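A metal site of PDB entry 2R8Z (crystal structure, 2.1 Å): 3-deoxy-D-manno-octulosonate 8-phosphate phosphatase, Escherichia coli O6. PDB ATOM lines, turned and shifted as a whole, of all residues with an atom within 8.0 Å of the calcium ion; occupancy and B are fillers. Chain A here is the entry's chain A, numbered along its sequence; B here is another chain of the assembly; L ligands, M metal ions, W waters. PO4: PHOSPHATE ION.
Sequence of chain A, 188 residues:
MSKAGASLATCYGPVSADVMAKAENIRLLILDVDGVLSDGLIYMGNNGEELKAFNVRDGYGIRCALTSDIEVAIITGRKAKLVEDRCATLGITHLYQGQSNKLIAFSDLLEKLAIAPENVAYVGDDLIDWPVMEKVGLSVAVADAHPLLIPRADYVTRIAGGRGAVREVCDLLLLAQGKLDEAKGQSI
The side-chain carboxylate (OD1) of Asp 32 lies within salt-bridge range of the side-chain amino group (NZ) of Lys 102 (3.1 Å).
The backbone NH of Asp 32 sits at hydrogen-bond distance from the backbone carbonyl oxygen of Val 123 (3.1 Å).
The side-chain carboxylate (OD2) of Asp 129 lies within hydrogen-bond range of the backbone NH (N) of Asp 125, at 3.1 Å.
OD1 of Asp 125 is in salt-bridge range of NH2 of Arg 57 of chain B, 2.9 Å away.
Of the 26 residues printed, 3 come within 4 Å of the calcium ion.
The nearest printed residue that does not touch the calcium ion is Asp 129 (4.1 Å).
OD2 of Asp 32 binds the calcium ion, at 2.2 Å.
The calcium ion is bound by water W1, 2.2 Å away.
The calcium ion is bound by the side-chain carboxylate (OD2) of Asp 125 (2.2 Å).
O4 of the ligand binds the calcium ion (2.3 Å).
The calcium ion is bound by O of Asp 34, at 2.3 Å.
The calcium ion is bound by water W2, at 2.4 Å.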
ATOM      1  N   LEU A  31      10.648  11.446  17.704  1.00  0.00           N
ATOM      2  CA  LEU A  31      11.827  10.603  17.686  1.00  0.00           C
ATOM      3  C   LEU A  31      12.277  10.250  19.087  1.00  0.00           C
ATOM      4  O   LEU A  31      12.305  11.080  20.002  1.00  0.00           O
ATOM      5  CB  LEU A  31      12.982  11.294  16.958  1.00  0.00           C
ATOM      6  CG  LEU A  31      12.710  11.885  15.570  1.00  0.00           C
ATOM      7  CD1 LEU A  31      13.834  12.851  15.172  1.00  0.00           C
ATOM      8  CD2 LEU A  31      12.560  10.772  14.523  1.00  0.00           C
ATOM      9  N   ASP A  32      12.619   8.983  19.244  1.00  0.00           N
ATOM     10  CA  ASP A  32      13.379   8.486  20.356  1.00  0.00           C
ATOM     11  C   ASP A  32      14.834   8.951  20.144  1.00  0.00           C
ATOM     12  O   ASP A  32      15.199   9.296  19.014  1.00  0.00           O
ATOM     13  CB  ASP A  32      13.271   6.971  20.263  1.00  0.00           C
ATOM     14  CG  ASP A  32      13.929   6.263  21.365  1.00  0.00           C
ATOM     15  OD1 ASP A  32      14.264   6.887  22.382  1.00  0.00           O
ATOM     16  OD2 ASP A  32      14.112   5.044  21.216  1.00  0.00           O
ATOM     17  N   VAL A  33      15.645   8.995  21.202  1.00  0.00           N
ATOM     18  CA  VAL A  33      17.044   9.411  21.024  1.00  0.00           C
ATOM     19  C   VAL A  33      17.970   8.203  20.943  1.00  0.00           C
ATOM     20  O   VAL A  33      18.541   7.911  19.878  1.00  0.00           O
ATOM     21  CB  VAL A  33      17.539  10.420  22.104  1.00  0.00           C
ATOM     22  CG1 VAL A  33      19.040  10.706  21.944  1.00  0.00           C
ATOM     23  CG2 VAL A  33      16.775  11.735  22.018  1.00  0.00           C
ATOM     24  N   ASP A  34      18.115   7.494  22.055  1.00  0.00           N
ATOM     25  CA  ASP A  34      19.057   6.383  22.130  1.00  0.00           C
ATOM     26  C   ASP A  34      18.597   5.213  21.262  1.00  0.00           C
ATOM     27  O   ASP A  34      17.510   4.664  21.462  1.00  0.00           O
ATOM     28  CB  ASP A  34      19.244   5.967  23.585  1.00  0.00           C
ATOM     29  CG  ASP A  34      19.838   7.083  24.444  1.00  0.00           C
ATOM     30  OD1 ASP A  34      20.952   7.551  24.129  1.00  0.00           O
ATOM     31  OD2 ASP A  34      19.178   7.498  25.417  1.00  0.00           O
ATOM     32  N   GLY A  35      19.421   4.874  20.266  1.00  0.00           N
ATOM     33  CA  GLY A  35      19.122   3.757  19.372  1.00  0.00           C
ATOM     34  C   GLY A  35      18.355   4.173  18.123  1.00  0.00           C
ATOM     35  O   GLY A  35      18.104   3.349  17.242  1.00  0.00           O
ATOM     36  N   VAL A  36      17.985   5.456  18.056  1.00  0.00           N
ATOM     37  CA  VAL A  36      17.294   6.035  16.895  1.00  0.00           C
ATOM     38  C   VAL A  36      18.138   7.167  16.280  1.00  0.00           C
ATOM     39  O   VAL A  36      18.602   7.038  15.148  1.00  0.00           O
ATOM     40  CB  VAL A  36      15.842   6.479  17.253  1.00  0.00           C
ATOM     41  CG1 VAL A  36      15.216   7.306  16.139  1.00  0.00           C
ATOM     42  CG2 VAL A  36      14.978   5.256  17.530  1.00  0.00           C
ATOM     43  N   LEU A  37      18.331   8.251  17.032  1.00  0.00           N
ATOM     44  CA  LEU A  37      19.269   9.310  16.646  1.00  0.00           C
ATOM     45  C   LEU A  37      20.737   8.944  16.921  1.00  0.00           C
ATOM     46  O   LEU A  37      21.651   9.562  16.368  1.00  0.00           O
ATOM     47  CB  LEU A  37      18.908  10.616  17.361  1.00  0.00           C
ATOM     48  CG  LEU A  37      17.647  11.319  16.857  1.00  0.00           C
ATOM     49  CD1 LEU A  37      17.215  12.348  17.868  1.00  0.00           C
ATOM     50  CD2 LEU A  37      17.896  11.960  15.499  1.00  0.00           C
ATOM     51  N   SER A  38      20.947   7.958  17.784  1.00  0.00           N
ATOM     52  CA  SER A  38      22.287   7.430  18.068  1.00  0.00           C
ATOM     53  C   SER A  38      22.284   5.936  17.805  1.00  0.00           C
ATOM     54  O   SER A  38      21.237   5.354  17.529  1.00  0.00           O
ATOM     55  CB  SER A  38      22.662   7.696  19.513  1.00  0.00           C
ATOM     56  OG  SER A  38      21.879   6.879  20.375  1.00  0.00           O
ATOM     57  N   GLY A  40      22.750   3.763  20.026  1.00  0.00           N
ATOM     58  CA  GLY A  40      22.374   3.133  21.289  1.00  0.00           C
ATOM     59  C   GLY A  40      23.443   3.135  22.371  1.00  0.00           C
ATOM     60  O   GLY A  40      23.210   2.638  23.467  1.00  0.00           O
ATOM     61  N   ILE A  75      11.180  12.517  22.454  1.00  0.00           N
ATOM     62  CA  ILE A  75      10.797  11.962  23.749  1.00  0.00           C
ATOM     63  C   ILE A  75      11.811  10.889  24.147  1.00  0.00           C
ATOM     64  O   ILE A  75      11.895   9.840  23.504  1.00  0.00           O
ATOM     65  CB  ILE A  75       9.365  11.359  23.747  1.00  0.00           C
ATOM     66  CG1 ILE A  75       8.315  12.412  23.338  1.00  0.00           C
ATOM     67  CG2 ILE A  75       9.023  10.792  25.117  1.00  0.00           C
ATOM     68  CD1 ILE A  75       6.923  11.831  23.040  1.00  0.00           C
ATOM     69  N   THR A  76      12.576  11.170  25.201  1.00  0.00           N
ATOM     70  CA  THR A  76      13.646  10.270  25.638  1.00  0.00           C
ATOM     71  C   THR A  76      13.547   9.930  27.133  1.00  0.00           C
ATOM     72  O   THR A  76      13.187  10.784  27.950  1.00  0.00           O
ATOM     73  CB  THR A  76      15.053  10.837  25.264  1.00  0.00           C
ATOM     74  OG1 THR A  76      16.078   9.966  25.755  1.00  0.00           O
ATOM     75  CG2 THR A  76      15.269  12.240  25.809  1.00  0.00           C
ATOM     76  N   GLY A  77      13.879   8.684  27.464  1.00  0.00           N
ATOM     77  CA  GLY A  77      13.858   8.222  28.842  1.00  0.00           C
ATOM     78  C   GLY A  77      15.027   8.709  29.674  1.00  0.00           C
ATOM     79  O   GLY A  77      14.951   8.761  30.892  1.00  0.00           O
ATOM     80  N   LYS A 102       6.115   7.427  28.064  1.00  0.00           N
ATOM     81  CA  LYS A 102       6.192   8.338  26.933  1.00  0.00           C
ATOM     82  C   LYS A 102       4.815   8.826  26.481  1.00  0.00           C
ATOM     83  O   LYS A 102       4.721   9.789  25.716  1.00  0.00           O
ATOM     84  CB  LYS A 102       6.971   7.679  25.783  1.00  0.00           C
ATOM     85  CG  LYS A 102       8.422   7.314  26.178  1.00  0.00           C
ATOM     86  CD  LYS A 102       9.270   6.972  24.959  1.00  0.00           C
ATOM     87  CE  LYS A 102      10.754   6.991  25.310  1.00  0.00           C
ATOM     88  NZ  LYS A 102      11.640   6.969  24.108  1.00  0.00           N
ATOM     89  N   TYR A 122       6.126   8.129  14.646  1.00  0.00           N
ATOM     90  CA  TYR A 122       7.029   7.881  15.760  1.00  0.00           C
ATOM     91  C   TYR A 122       8.092   6.859  15.365  1.00  0.00           C
ATOM     92  O   TYR A 122       7.756   5.769  14.890  1.00  0.00           O
ATOM     93  CB  TYR A 122       6.276   7.402  17.017  1.00  0.00           C
ATOM     94  CG  TYR A 122       7.134   7.359  18.271  1.00  0.00           C
ATOM     95  CD1 TYR A 122       6.979   8.315  19.272  1.00  0.00           C
ATOM     96  CD2 TYR A 122       8.121   6.384  18.437  1.00  0.00           C
ATOM     97  CE1 TYR A 122       7.775   8.286  20.426  1.00  0.00           C
ATOM     98  CE2 TYR A 122       8.920   6.341  19.557  1.00  0.00           C
ATOM     99  CZ  TYR A 122       8.744   7.292  20.555  1.00  0.00           C
ATOM    100  OH  TYR A 122       9.544   7.238  21.676  1.00  0.00           O
ATOM    101  N   VAL A 123       9.351   7.222  15.573  1.00  0.00           N
ATOM    102  CA  VAL A 123      10.472   6.311  15.301  1.00  0.00           C
ATOM    103  C   VAL A 123      11.091   5.849  16.608  1.00  0.00           C
ATOM    104  O   VAL A 123      11.594   6.666  17.392  1.00  0.00           O
ATOM    105  CB  VAL A 123      11.564   6.975  14.400  1.00  0.00           C
ATOM    106  CG1 VAL A 123      12.562   5.928  13.927  1.00  0.00           C
ATOM    107  CG2 VAL A 123      10.919   7.672  13.188  1.00  0.00           C
ATOM    108  N   GLY A 124      11.039   4.540  16.877  1.00  0.00           N
ATOM    109  CA  GLY A 124      11.555   3.963  18.115  1.00  0.00           C
ATOM    110  C   GLY A 124      12.420   2.723  17.898  1.00  0.00           C
ATOM    111  O   GLY A 124      12.444   2.180  16.806  1.00  0.00           O
ATOM    112  N   ASP A 125      13.103   2.283  18.949  1.00  0.00           N
ATOM    113  CA  ASP A 125      13.928   1.069  18.837  1.00  0.00           C
ATOM    114  C   ASP A 125      13.690   0.010  19.908  1.00  0.00           C
ATOM    115  O   ASP A 125      14.222  -1.104  19.798  1.00  0.00           O
ATOM    116  CB  ASP A 125      15.429   1.418  18.761  1.00  0.00           C
ATOM    117  CG  ASP A 125      16.028   1.741  20.102  1.00  0.00           C
ATOM    118  OD1 ASP A 125      17.186   1.304  20.375  1.00  0.00           O
ATOM    119  OD2 ASP A 125      15.344   2.428  20.908  1.00  0.00           O
ATOM    120  N   ASP A 126      12.899   0.330  20.937  1.00  0.00           N
ATOM    121  CA  ASP A 126      12.673  -0.620  22.031  1.00  0.00           C
ATOM    122  C   ASP A 126      11.216  -0.681  22.486  1.00  0.00           C
ATOM    123  O   ASP A 126      10.388   0.167  22.100  1.00  0.00           O
ATOM    124  CB  ASP A 126      13.599  -0.324  23.227  1.00  0.00           C
ATOM    125  CG  ASP A 126      13.990  -1.569  24.014  1.00  0.00           C
ATOM    126  OD1 ASP A 126      13.445  -2.660  23.725  1.00  0.00           O
ATOM    127  OD2 ASP A 126      14.844  -1.462  24.921  1.00  0.00           O
ATOM    128  N   LEU A 127      10.893  -1.679  23.300  1.00  0.00           N
ATOM    129  CA  LEU A 127       9.511  -1.970  23.694  1.00  0.00           C
ATOM    130  C   LEU A 127       8.812  -0.829  24.437  1.00  0.00           C
ATOM    131  O   LEU A 127       7.606  -0.641  24.319  1.00  0.00           O
ATOM    132  CB  LEU A 127       9.443  -3.262  24.503  1.00  0.00           C
ATOM    133  CG  LEU A 127      10.148  -4.471  23.858  1.00  0.00           C
ATOM    134  CD1 LEU A 127      10.096  -5.684  24.775  1.00  0.00           C
ATOM    135  CD2 LEU A 127       9.573  -4.804  22.485  1.00  0.00           C
ATOM    136  N   ILE A 128       9.601  -0.047  25.179  1.00  0.00           N
ATOM    137  CA  ILE A 128       9.103   1.136  25.899  1.00  0.00           C
ATOM    138  C   ILE A 128       8.492   2.208  24.965  1.00  0.00           C
ATOM    139  O   ILE A 128       7.736   3.067  25.403  1.00  0.00           O
ATOM    140  CB  ILE A 128      10.212   1.707  26.837  1.00  0.00           C
ATOM    141  CG1 ILE A 128       9.636   2.639  27.908  1.00  0.00           C
ATOM    142  CG2 ILE A 128      11.328   2.388  26.023  1.00  0.00           C
ATOM    143  CD1 ILE A 128       8.582   1.981  28.786  1.00  0.00           C
ATOM    144  N   ASP A 129       8.824   2.122  23.675  1.00  0.00           N
ATOM    145  CA  ASP A 129       8.312   3.062  22.673  1.00  0.00           C
ATOM    146  C   ASP A 129       6.960   2.662  22.116  1.00  0.00           C
ATOM    147  O   ASP A 129       6.209   3.512  21.613  1.00  0.00           O
ATOM    148  CB  ASP A 129       9.304   3.194  21.519  1.00  0.00           C
ATOM    149  CG  ASP A 129      10.622   3.788  21.960  1.00  0.00           C
ATOM    150  OD1 ASP A 129      10.606   4.766  22.741  1.00  0.00           O
ATOM    151  OD2 ASP A 129      11.671   3.284  21.528  1.00  0.00           O
ATOM    152  N   VAL A 142      13.492   1.240  13.784  1.00  0.00           N
ATOM    153  CA  VAL A 142      14.776   1.249  13.072  1.00  0.00           C
ATOM    154  C   VAL A 142      15.181  -0.194  12.729  1.00  0.00           C
ATOM    155  O   VAL A 142      14.634  -1.139  13.313  1.00  0.00           O
ATOM    156  CB  VAL A 142      15.889   2.003  13.823  1.00  0.00           C
ATOM    157  CG1 VAL A 142      15.504   3.471  14.011  1.00  0.00           C
ATOM    158  CG2 VAL A 142      16.197   1.354  15.186  1.00  0.00           C
ATOM    159  N   VAL B  56      22.183   1.229  25.881  1.00  0.00           N
ATOM    160  CA  VAL B  56      20.964   1.529  26.630  1.00  0.00           C
ATOM    161  C   VAL B  56      19.957   0.371  26.623  1.00  0.00           C
ATOM    162  O   VAL B  56      19.226   0.200  27.588  1.00  0.00           O
ATOM    163  CB  VAL B  56      20.254   2.851  26.197  1.00  0.00           C
ATOM    164  CG1 VAL B  56      21.214   4.002  26.148  1.00  0.00           C
ATOM    165  CG2 VAL B  56      19.570   2.699  24.885  1.00  0.00           C
ATOM    166  N   ARG B  57      19.937  -0.398  25.535  1.00  0.00           N
ATOM    167  CA  ARG B  57      19.069  -1.574  25.475  1.00  0.00           C
ATOM    168  C   ARG B  57      19.512  -2.677  26.454  1.00  0.00           C
ATOM    169  O   ARG B  57      18.667  -3.401  26.953  1.00  0.00           O
ATOM    170  CB  ARG B  57      18.891  -2.084  24.035  1.00  0.00           C
ATOM    171  CG  ARG B  57      18.102  -1.091  23.127  1.00  0.00           C
ATOM    172  CD  ARG B  57      17.119  -1.808  22.198  1.00  0.00           C
ATOM    173  NE  ARG B  57      17.760  -2.783  21.313  1.00  0.00           N
ATOM    174  CZ  ARG B  57      18.113  -2.561  20.053  1.00  0.00           C
ATOM    175  NH1 ARG B  57      18.679  -3.539  19.357  1.00  0.00           N
ATOM    176  NH2 ARG B  57      17.885  -1.376  19.479  1.00  0.00           N
ATOM    177  N   SER B 187      14.876   2.387  29.805  1.00  0.00           N
ATOM    178  CA  SER B 187      15.881   2.442  28.742  1.00  0.00           C
ATOM    179  C   SER B 187      16.912   3.521  29.051  1.00  0.00           C
ATOM    180  O   SER B 187      16.762   4.683  28.635  1.00  0.00           O
ATOM    181  CB  SER B 187      15.210   2.711  27.398  1.00  0.00           C
ATOM    182  OG  SER B 187      14.128   3.613  27.540  1.00  0.00           O
ATOM    183  N   ILE B 188      17.947   3.119  29.794  1.00  0.00           N
ATOM    184  CA  ILE B 188      18.962   4.038  30.317  1.00  0.00           C
ATOM    185  C   ILE B 188      20.396   3.503  30.160  1.00  0.00           C
ATOM    186  O   ILE B 188      20.637   2.312  29.965  1.00  0.00           O
ATOM    187  CB  ILE B 188      18.708   4.417  31.817  1.00  0.00           C
ATOM    188  CG1 ILE B 188      18.604   3.155  32.687  1.00  0.00           C
ATOM    189  CG2 ILE B 188      17.453   5.319  31.941  1.00  0.00           C
ATOM    190  CD1 ILE B 188      18.384   3.417  34.173  1.00  0.00           C
ATOM    191  OXT ILE B 188      21.367   4.255  30.209  1.00  0.00           O
HETATM  192  P   PO4 L   1      15.626   6.850  24.935  1.00  0.00           P
HETATM  193  O1  PO4 L   1      16.628   6.720  26.067  1.00  0.00           O
HETATM  194  O2  PO4 L   1      14.198   6.801  25.434  1.00  0.00           O
HETATM  195  O3  PO4 L   1      15.934   8.021  24.042  1.00  0.00           O
HETATM  196  O4  PO4 L   1      15.671   5.662  24.003  1.00  0.00           O
HETATM  197 CA    CA M   1      15.580   4.020  22.460  1.00  0.00          CA
HETATM  198  O   HOH W   1      16.757   2.776  23.858  1.00  0.00           O
HETATM  199  O   HOH W   2      13.735   3.333  23.764  1.00  0.00           O
